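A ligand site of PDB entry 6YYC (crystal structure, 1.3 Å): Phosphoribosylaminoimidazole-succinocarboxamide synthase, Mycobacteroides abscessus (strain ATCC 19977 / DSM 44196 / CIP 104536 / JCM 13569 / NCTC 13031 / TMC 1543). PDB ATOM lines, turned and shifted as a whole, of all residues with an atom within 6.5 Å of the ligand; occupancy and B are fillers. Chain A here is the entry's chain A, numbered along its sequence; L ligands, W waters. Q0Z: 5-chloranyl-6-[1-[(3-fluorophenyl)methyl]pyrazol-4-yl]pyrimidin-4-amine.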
ATOM      1  N   HIS A  19      26.085  20.785   3.401  1.00  0.00           N
ATOM      2  CA  HIS A  19      26.656  21.823   4.250  1.00  0.00           C
ATOM      3  C   HIS A  19      25.633  22.925   4.476  1.00  0.00           C
ATOM      4  O   HIS A  19      25.064  23.451   3.516  1.00  0.00           O
ATOM      5  CB  HIS A  19      27.925  22.378   3.608  1.00  0.00           C
ATOM      6  CG  HIS A  19      28.602  23.444   4.406  1.00  0.00           C
ATOM      7  ND1 HIS A  19      28.893  24.690   3.882  1.00  0.00           N
ATOM      8  CD2 HIS A  19      29.071  23.452   5.674  1.00  0.00           C
ATOM      9  CE1 HIS A  19      29.505  25.410   4.804  1.00  0.00           C
ATOM     10  NE2 HIS A  19      29.631  24.693   5.896  1.00  0.00           N
ATOM     11  N   VAL A  20      25.392  23.259   5.740  1.00  0.00           N
ATOM     12  CA  VAL A  20      24.417  24.313   6.053  1.00  0.00           C
ATOM     13  C   VAL A  20      24.995  25.495   6.825  1.00  0.00           C
ATOM     14  O   VAL A  20      24.412  26.577   6.828  1.00  0.00           O
ATOM     15  CB  VAL A  20      23.196  23.781   6.851  1.00  0.00           C
ATOM     16  CG1 VAL A  20      22.365  22.855   5.995  1.00  0.00           C
ATOM     17  CG2 VAL A  20      23.636  23.099   8.144  1.00  0.00           C
ATOM     18  N   ALA A  21      26.125  25.305   7.496  1.00  0.00           N
ATOM     19  CA  ALA A  21      26.739  26.392   8.242  1.00  0.00           C
ATOM     20  C   ALA A  21      28.223  26.178   8.479  1.00  0.00           C
ATOM     21  O   ALA A  21      28.685  25.040   8.561  1.00  0.00           O
ATOM     22  CB  ALA A  21      26.036  26.585   9.583  1.00  0.00           C
ATOM     23  N   SER A  22      28.942  27.281   8.595  1.00  0.00           N
ATOM     24  CA  SER A  22      30.342  27.274   8.973  1.00  0.00           C
ATOM     25  C   SER A  22      30.634  28.345  10.017  1.00  0.00           C
ATOM     26  O   SER A  22      30.153  29.473   9.904  1.00  0.00           O
ATOM     27  CB  SER A  22      31.235  27.489   7.759  1.00  0.00           C
ATOM     28  OG  SER A  22      31.382  26.293   7.020  1.00  0.00           O
ATOM     29  N   GLY A  23      31.414  27.978  11.020  1.00  0.00           N
ATOM     30  CA  GLY A  23      31.962  28.931  11.970  1.00  0.00           C
ATOM     31  C   GLY A  23      33.449  28.986  11.750  1.00  0.00           C
ATOM     32  O   GLY A  23      33.968  28.345  10.821  1.00  0.00           O
ATOM     33  N   LYS A  24      34.141  29.729  12.597  1.00  0.00           N
ATOM     34  CA  LYS A  24      35.585  29.882  12.458  1.00  0.00           C
ATOM     35  C   LYS A  24      36.336  28.542  12.478  1.00  0.00           C
ATOM     36  O   LYS A  24      37.287  28.339  11.730  1.00  0.00           O
ATOM     37  CB  LYS A  24      36.120  30.802  13.552  1.00  0.00           C
ATOM     38  N   ARG A  26      34.421  25.354  13.159  1.00  0.00           N
ATOM     39  CA  ARG A  26      33.455  24.264  13.172  1.00  0.00           C
ATOM     40  C   ARG A  26      32.552  24.339  11.952  1.00  0.00           C
ATOM     41  O   ARG A  26      32.456  25.379  11.283  1.00  0.00           O
ATOM     42  CB  ARG A  26      32.614  24.288  14.460  1.00  0.00           C
ATOM     43  CG  ARG A  26      31.877  25.584  14.687  1.00  0.00           C
ATOM     44  CD  ARG A  26      31.251  25.593  16.064  1.00  0.00           C
ATOM     45  NE  ARG A  26      30.331  26.701  16.218  1.00  0.00           N
ATOM     46  CZ  ARG A  26      29.585  26.886  17.296  1.00  0.00           C
ATOM     47  NH1 ARG A  26      29.695  26.038  18.315  1.00  0.00           N
ATOM     48  NH2 ARG A  26      28.744  27.909  17.366  1.00  0.00           N
ATOM     49  N   GLU A  27      31.877  23.226  11.643  1.00  0.00           N
ATOM     50  CA  GLU A  27      31.018  23.136  10.474  1.00  0.00           C
ATOM     51  C   GLU A  27      29.730  22.402  10.837  1.00  0.00           C
ATOM     52  O   GLU A  27      29.727  21.621  11.779  1.00  0.00           O
ATOM     53  CB  GLU A  27      31.728  22.402   9.326  1.00  0.00           C
ATOM     54  CG  GLU A  27      33.010  23.036   8.860  1.00  0.00           C
ATOM     55  CD  GLU A  27      33.757  22.149   7.898  1.00  0.00           C
ATOM     56  OE1 GLU A  27      33.547  20.918   7.918  1.00  0.00           O
ATOM     57  OE2 GLU A  27      34.546  22.691   7.102  1.00  0.00           O
ATOM     58  N   LEU A  28      28.685  22.612  10.048  1.00  0.00           N
ATOM     59  CA  LEU A  28      27.399  21.966  10.299  1.00  0.00           C
ATOM     60  C   LEU A  28      26.824  21.393   8.995  1.00  0.00           C
ATOM     61  O   LEU A  28      26.834  22.043   7.954  1.00  0.00           O
ATOM     62  CB  LEU A  28      26.419  22.948  10.945  1.00  0.00           C
ATOM     63  CG  LEU A  28      25.127  22.412  11.547  1.00  0.00           C
ATOM     64  CD1 LEU A  28      25.410  21.431  12.690  1.00  0.00           C
ATOM     65  CD2 LEU A  28      24.249  23.575  12.012  1.00  0.00           C
ATOM     66  N   LEU A  36      21.278  16.713  12.185  1.00  0.00           N
ATOM     67  CA  LEU A  36      22.447  17.389  11.643  1.00  0.00           C
ATOM     68  C   LEU A  36      23.726  16.691  12.077  1.00  0.00           C
ATOM     69  O   LEU A  36      23.724  15.850  12.979  1.00  0.00           O
ATOM     70  CB  LEU A  36      22.461  18.850  12.091  1.00  0.00           C
ATOM     71  CG  LEU A  36      21.144  19.632  11.991  1.00  0.00           C
ATOM     72  CD1 LEU A  36      21.297  21.004  12.627  1.00  0.00           C
ATOM     73  CD2 LEU A  36      20.689  19.741  10.554  1.00  0.00           C
ATOM     74  N   LEU A  37      24.818  17.051  11.405  1.00  0.00           N
ATOM     75  CA  LEU A  37      26.155  16.583  11.756  1.00  0.00           C
ATOM     76  C   LEU A  37      26.969  17.789  12.209  1.00  0.00           C
ATOM     77  O   LEU A  37      27.195  18.716  11.435  1.00  0.00           O
ATOM     78  CB  LEU A  37      26.828  15.898  10.565  1.00  0.00           C
ATOM     79  CG  LEU A  37      28.167  15.260  10.889  1.00  0.00           C
ATOM     80  CD1 LEU A  37      27.980  14.005  11.708  1.00  0.00           C
ATOM     81  CD2 LEU A  37      28.958  14.958   9.609  1.00  0.00           C
ATOM     82  N   PHE A  38      27.370  17.770  13.469  1.00  0.00           N
ATOM     83  CA  PHE A  38      28.032  18.887  14.148  1.00  0.00           C
ATOM     84  C   PHE A  38      29.536  18.574  14.143  1.00  0.00           C
ATOM     85  O   PHE A  38      29.983  17.684  14.854  1.00  0.00           O
ATOM     86  CB  PHE A  38      27.471  19.019  15.578  1.00  0.00           C
ATOM     87  CG  PHE A  38      27.766  20.320  16.259  1.00  0.00           C
ATOM     88  CD1 PHE A  38      29.053  20.688  16.609  1.00  0.00           C
ATOM     89  CD2 PHE A  38      26.719  21.154  16.631  1.00  0.00           C
ATOM     90  CE1 PHE A  38      29.283  21.888  17.273  1.00  0.00           C
ATOM     91  CE2 PHE A  38      26.938  22.350  17.301  1.00  0.00           C
ATOM     92  CZ  PHE A  38      28.228  22.717  17.623  1.00  0.00           C
ATOM     93  N   VAL A  39      30.312  19.317  13.356  1.00  0.00           N
ATOM     94  CA  VAL A  39      31.713  18.964  13.095  1.00  0.00           C
ATOM     95  C   VAL A  39      32.719  19.965  13.679  1.00  0.00           C
ATOM     96  O   VAL A  39      32.673  21.161  13.374  1.00  0.00           O
ATOM     97  CB  VAL A  39      31.972  18.831  11.572  1.00  0.00           C
ATOM     98  CG1 VAL A  39      33.429  18.478  11.291  1.00  0.00           C
ATOM     99  CG2 VAL A  39      31.024  17.805  10.955  1.00  0.00           C
ATOM    100  N   HIS A  78      21.208  17.966  22.637  1.00  0.00           N
ATOM    101  CA  HIS A  78      20.788  17.713  21.282  1.00  0.00           C
ATOM    102  C   HIS A  78      21.474  16.491  20.657  1.00  0.00           C
ATOM    103  O   HIS A  78      21.189  16.164  19.525  1.00  0.00           O
ATOM    104  CB  HIS A  78      20.997  19.001  20.464  1.00  0.00           C
ATOM    105  CG  HIS A  78      22.418  19.324  20.077  1.00  0.00           C
ATOM    106  ND1 HIS A  78      23.542  18.979  20.835  1.00  0.00           N
ATOM    107  CD2 HIS A  78      22.888  20.110  19.094  1.00  0.00           C
ATOM    108  CE1 HIS A  78      24.616  19.455  20.262  1.00  0.00           C
ATOM    109  NE2 HIS A  78      24.264  20.177  19.208  1.00  0.00           N
ATOM    110  N   VAL A  99      23.301  15.114  15.739  1.00  0.00           N
ATOM    111  CA  VAL A  99      22.457  15.863  16.674  1.00  0.00           C
ATOM    112  C   VAL A  99      21.040  16.045  16.134  1.00  0.00           C
ATOM    113  O   VAL A  99      20.807  15.973  14.946  1.00  0.00           O
ATOM    114  CB  VAL A  99      23.078  17.250  17.012  1.00  0.00           C
ATOM    115  CG1 VAL A  99      24.482  17.099  17.599  1.00  0.00           C
ATOM    116  CG2 VAL A  99      23.106  18.147  15.781  1.00  0.00           C
ATOM    117  N   ARG A 100      20.095  16.273  17.039  1.00  0.00           N
ATOM    118  CA  ARG A 100      18.707  16.526  16.649  1.00  0.00           C
ATOM    119  C   ARG A 100      18.549  17.937  16.130  1.00  0.00           C
ATOM    120  O   ARG A 100      19.089  18.850  16.731  1.00  0.00           O
ATOM    121  CB  ARG A 100      17.748  16.356  17.823  1.00  0.00           C
ATOM    122  CG  ARG A 100      17.639  14.986  18.444  1.00  0.00           C
ATOM    123  CD  ARG A 100      16.556  15.034  19.539  1.00  0.00           C
ATOM    124  NE  ARG A 100      17.043  15.630  20.793  1.00  0.00           N
ATOM    125  CZ  ARG A 100      16.279  16.256  21.689  1.00  0.00           C
ATOM    126  NH1 ARG A 100      16.825  16.748  22.799  1.00  0.00           N
ATOM    127  NH2 ARG A 100      14.980  16.394  21.482  1.00  0.00           N
ATOM    128  N   ARG A 101      17.802  18.129  15.055  1.00  0.00           N
ATOM    129  CA  ARG A 101      17.546  19.484  14.583  1.00  0.00           C
ATOM    130  C   ARG A 101      16.526  20.121  15.513  1.00  0.00           C
ATOM    131  O   ARG A 101      15.503  19.526  15.828  1.00  0.00           O
ATOM    132  CB  ARG A 101      17.024  19.506  13.149  1.00  0.00           C
ATOM    133  CG  ARG A 101      16.880  20.920  12.611  1.00  0.00           C
ATOM    134  CD  ARG A 101      16.156  20.964  11.282  1.00  0.00           C
ATOM    135  NE  ARG A 101      14.962  20.123  11.292  1.00  0.00           N
ATOM    136  CZ  ARG A 101      13.800  20.486  11.837  1.00  0.00           C
ATOM    137  NH1 ARG A 101      13.665  21.668  12.414  1.00  0.00           N
ATOM    138  NH2 ARG A 101      12.770  19.646  11.799  1.00  0.00           N
ATOM    139  N   LEU A 102      16.810  21.356  15.911  1.00  0.00           N
ATOM    140  CA  LEU A 102      16.012  22.122  16.851  1.00  0.00           C
ATOM    141  C   LEU A 102      15.693  23.521  16.324  1.00  0.00           C
ATOM    142  O   LEU A 102      16.358  24.006  15.428  1.00  0.00           O
ATOM    143  CB  LEU A 102      16.756  22.234  18.174  1.00  0.00           C
ATOM    144  CG  LEU A 102      17.072  20.959  18.944  1.00  0.00           C
ATOM    145  CD1 LEU A 102      18.138  21.240  20.011  1.00  0.00           C
ATOM    146  CD2 LEU A 102      15.821  20.381  19.590  1.00  0.00           C
ATOM    147  N   ASP A 103      14.681  24.168  16.904  1.00  0.00           N
ATOM    148  CA  ASP A 103      14.478  25.575  16.623  1.00  0.00           C
ATOM    149  C   ASP A 103      15.395  26.356  17.563  1.00  0.00           C
ATOM    150  O   ASP A 103      15.152  26.442  18.769  1.00  0.00           O
ATOM    151  CB  ASP A 103      13.019  25.981  16.830  1.00  0.00           C
ATOM    152  CG  ASP A 103      12.101  25.385  15.772  1.00  0.00           C
ATOM    153  OD1 ASP A 103      12.603  25.062  14.681  1.00  0.00           O
ATOM    154  OD2 ASP A 103      10.894  25.250  16.051  1.00  0.00           O
ATOM    155  N   MET A 104      16.465  26.894  17.008  1.00  0.00           N
ATOM    156  CA  MET A 104      17.450  27.564  17.821  1.00  0.00           C
ATOM    157  C   MET A 104      16.955  28.903  18.346  1.00  0.00           C
ATOM    158  O   MET A 104      16.283  29.654  17.646  1.00  0.00           O
ATOM    159  CB  MET A 104      18.738  27.763  17.036  1.00  0.00           C
ATOM    160  CG  MET A 104      19.346  26.415  16.664  1.00  0.00           C
ATOM    161  SD  MET A 104      19.798  25.349  18.043  1.00  0.00           S
ATOM    162  CE  MET A 104      21.163  26.263  18.748  1.00  0.00           C
ATOM    163  N   GLU A 209      24.529  27.955  23.093  1.00  0.00           N
ATOM    164  CA  GLU A 209      23.211  28.216  22.541  1.00  0.00           C
ATOM    165  C   GLU A 209      22.270  27.095  22.924  1.00  0.00           C
ATOM    166  O   GLU A 209      22.698  25.950  23.124  1.00  0.00           O
ATOM    167  CB  GLU A 209      23.256  28.370  21.023  1.00  0.00           C
ATOM    168  CG  GLU A 209      24.080  29.550  20.499  1.00  0.00           C
ATOM    169  CD  GLU A 209      24.399  29.449  19.005  1.00  0.00           C
ATOM    170  OE1 GLU A 209      24.179  28.372  18.401  1.00  0.00           O
ATOM    171  OE2 GLU A 209      24.888  30.434  18.422  1.00  0.00           O
ATOM    172  N   ALA A 221      22.305  22.892  22.949  1.00  0.00           N
ATOM    173  CA  ALA A 221      22.559  22.555  21.551  1.00  0.00           C
ATOM    174  C   ALA A 221      23.767  23.301  21.005  1.00  0.00           C
ATOM    175  O   ALA A 221      23.638  24.191  20.153  1.00  0.00           O
ATOM    176  CB  ALA A 221      21.316  22.874  20.692  1.00  0.00           C
ATOM    177  N   ASP A 222      24.940  22.935  21.498  1.00  0.00           N
ATOM    178  CA  ASP A 222      26.168  23.611  21.159  1.00  0.00           C
ATOM    179  C   ASP A 222      27.324  22.697  21.521  1.00  0.00           C
ATOM    180  O   ASP A 222      27.125  21.584  22.024  1.00  0.00           O
ATOM    181  CB  ASP A 222      26.270  24.928  21.926  1.00  0.00           C
ATOM    182  CG  ASP A 222      27.035  26.013  21.185  1.00  0.00           C
ATOM    183  OD1 ASP A 222      28.042  25.699  20.479  1.00  0.00           O
ATOM    184  OD2 ASP A 222      26.645  27.190  21.325  1.00  0.00           O
ATOM    185  N   GLU A 223      28.533  23.154  21.283  1.00  0.00           N
ATOM    186  CA  GLU A 223      29.664  22.509  21.929  1.00  0.00           C
ATOM    187  C   GLU A 223      29.618  23.033  23.347  1.00  0.00           C
ATOM    188  O   GLU A 223      29.197  24.178  23.591  1.00  0.00           O
ATOM    189  CB  GLU A 223      30.983  22.841  21.234  1.00  0.00           C
ATOM    190  CG  GLU A 223      31.380  24.290  21.322  1.00  0.00           C
ATOM    191  CD  GLU A 223      32.525  24.602  20.410  1.00  0.00           C
ATOM    192  OE1 GLU A 223      33.680  24.668  20.893  1.00  0.00           O
ATOM    193  OE2 GLU A 223      32.275  24.782  19.206  1.00  0.00           O
HETATM  194  C10 Q0Z L   1      23.735  25.525  15.433  1.00  0.00           C
HETATM  195  C13 Q0Z L   1      26.690  26.317  14.532  1.00  0.00           C
HETATM  196  C15 Q0Z L   1      28.248  25.886  12.760  1.00  0.00           C
HETATM  197  C17 Q0Z L   1      28.100  24.322  14.616  1.00  0.00           C
HETATM  198  C21 Q0Z L   1      22.555  26.024  13.594  1.00  0.00           C
HETATM  199  N01 Q0Z L   1      20.817  21.075  17.097  1.00  0.00           N
HETATM  200  C02 Q0Z L   1      20.705  22.161  16.158  1.00  0.00           C
HETATM  201  N03 Q0Z L   1      19.583  22.287  15.441  1.00  0.00           N
HETATM  202  C04 Q0Z L   1      19.435  23.286  14.574  1.00  0.00           C
HETATM  203  N05 Q0Z L   1      20.406  24.140  14.367  1.00  0.00           N
HETATM  204  C06 Q0Z L   1      21.574  24.105  15.021  1.00  0.00           C
HETATM  205  C07 Q0Z L   1      21.777  23.055  15.971  1.00  0.00           C
HETATM  206 CL1  Q0Z L   1      23.227  22.871  16.902  1.00  0.00          CL
HETATM  207  C09 Q0Z L   1      22.613  25.183  14.698  1.00  0.00           C
HETATM  208  N11 Q0Z L   1      24.333  26.525  14.779  1.00  0.00           N
HETATM  209  C12 Q0Z L   1      25.569  27.165  15.179  1.00  0.00           C
HETATM  210  C14 Q0Z L   1      27.251  26.704  13.319  1.00  0.00           C
HETATM  211  C16 Q0Z L   1      28.680  24.709  13.391  1.00  0.00           C
HETATM  212  C18 Q0Z L   1      27.103  25.139  15.175  1.00  0.00           C
HETATM  213  F19 Q0Z L   1      28.812  26.232  11.614  1.00  0.00           F
HETATM  214  N20 Q0Z L   1      23.646  26.847  13.663  1.00  0.00           N
HETATM  215  O   HOH W   1      24.125  28.920  11.620  1.00  0.00           O
HETATM  216  O   HOH W   2      19.260  26.451  13.167  1.00  0.00           O
HETATM  217  O   HOH W   3      25.233  25.644  18.401  1.00  0.00           O
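The backbone NH (N) of Glu 209 lies within hydrogen-bond range of the side-chain carboxylate (OD2) of Asp 222 (2.9 Å).
The backbone NH of Glu 27 is in hydrogen-bond range of the backbone carbonyl oxygen of Val 39 (2.8 Å).
The backbone NH of Arg 100 lies within hydrogen-bond range of the backbone carbonyl oxygen of His 78 (2.7 Å).
The backbone NH of Val 20 is in hydrogen-bond range of the backbone carbonyl oxygen of Leu 28 (2.9 Å).
The side-chain carboxylate (OE2) of Glu 223 lies within salt-bridge range of the guanidinium group (NH1) of Arg 26 (3.0 Å).
The backbone carbonyl oxygen (O) of Ala 21 is in hydrogen-bond range of the backbone NH (N) of Leu 28 (2.8 Å).
The backbone carbonyl oxygen of Ala 21 sits at hydrogen-bond distance from a ring nitrogen (NE2) of His 19 (2.8 Å).
The guanidinium group (NH1) of Arg 26 is in salt-bridge range of the side-chain carboxylate (OD1) of Asp 222 (2.7 Å).
N03 of the ligand lies within hydrogen-bond range of N of Leu 102 (3.0 Å).
The backbone carbonyl oxygen (O) of Arg 100 is in hydrogen-bond range of a nitrogen (N01) of the ligand, 2.8 Å away.
A fluorine (F19) of the ligand sits close to the backbone carbonyl oxygen of Ala 21 (3.3 Å).
F19 of the ligand sits close to N of Ser 22, at 3.2 Å.
F19 of the ligand lies close to N of Gly 23, 3.2 Å away.
Arg 26 touches the ligand.
Glu 27 touches the ligand.
Leu 28 touches the ligand.
Leu 36 touches the ligand.
CZ of Phe 38 touches C17 of the ligand, at 3.4 Å.
CD2 of His 78 touches N01 of the ligand, at 3.0 Å.
Val 99 touches the ligand.
Arg 101 touches the ligand (CA to N03, 3.6 Å).
Met 104 touches the ligand (CG to N05, 3.4 Å).
OE1 of Glu 209 touches C12 of the ligand, at 3.7 Å.
Ala 221 touches the ligand.
Hydrophobic or aromatic side chains that line the ligand: Ala 21, Leu 28, Leu 36, Phe 38, His 78, Val 99, Leu 102 and Met 104.
Within 4 Å of the ligand: Ala 21, Ser 22, Gly 23, Arg 26, Glu 27, Leu 28, Leu 36, Phe 38, His 78, Val 99, Arg 100, Arg 101, Leu 102, Met 104, Glu 209 and Ala 221.
Along chain A the residues within 4 Å of the ligand span positions 21 to 221.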
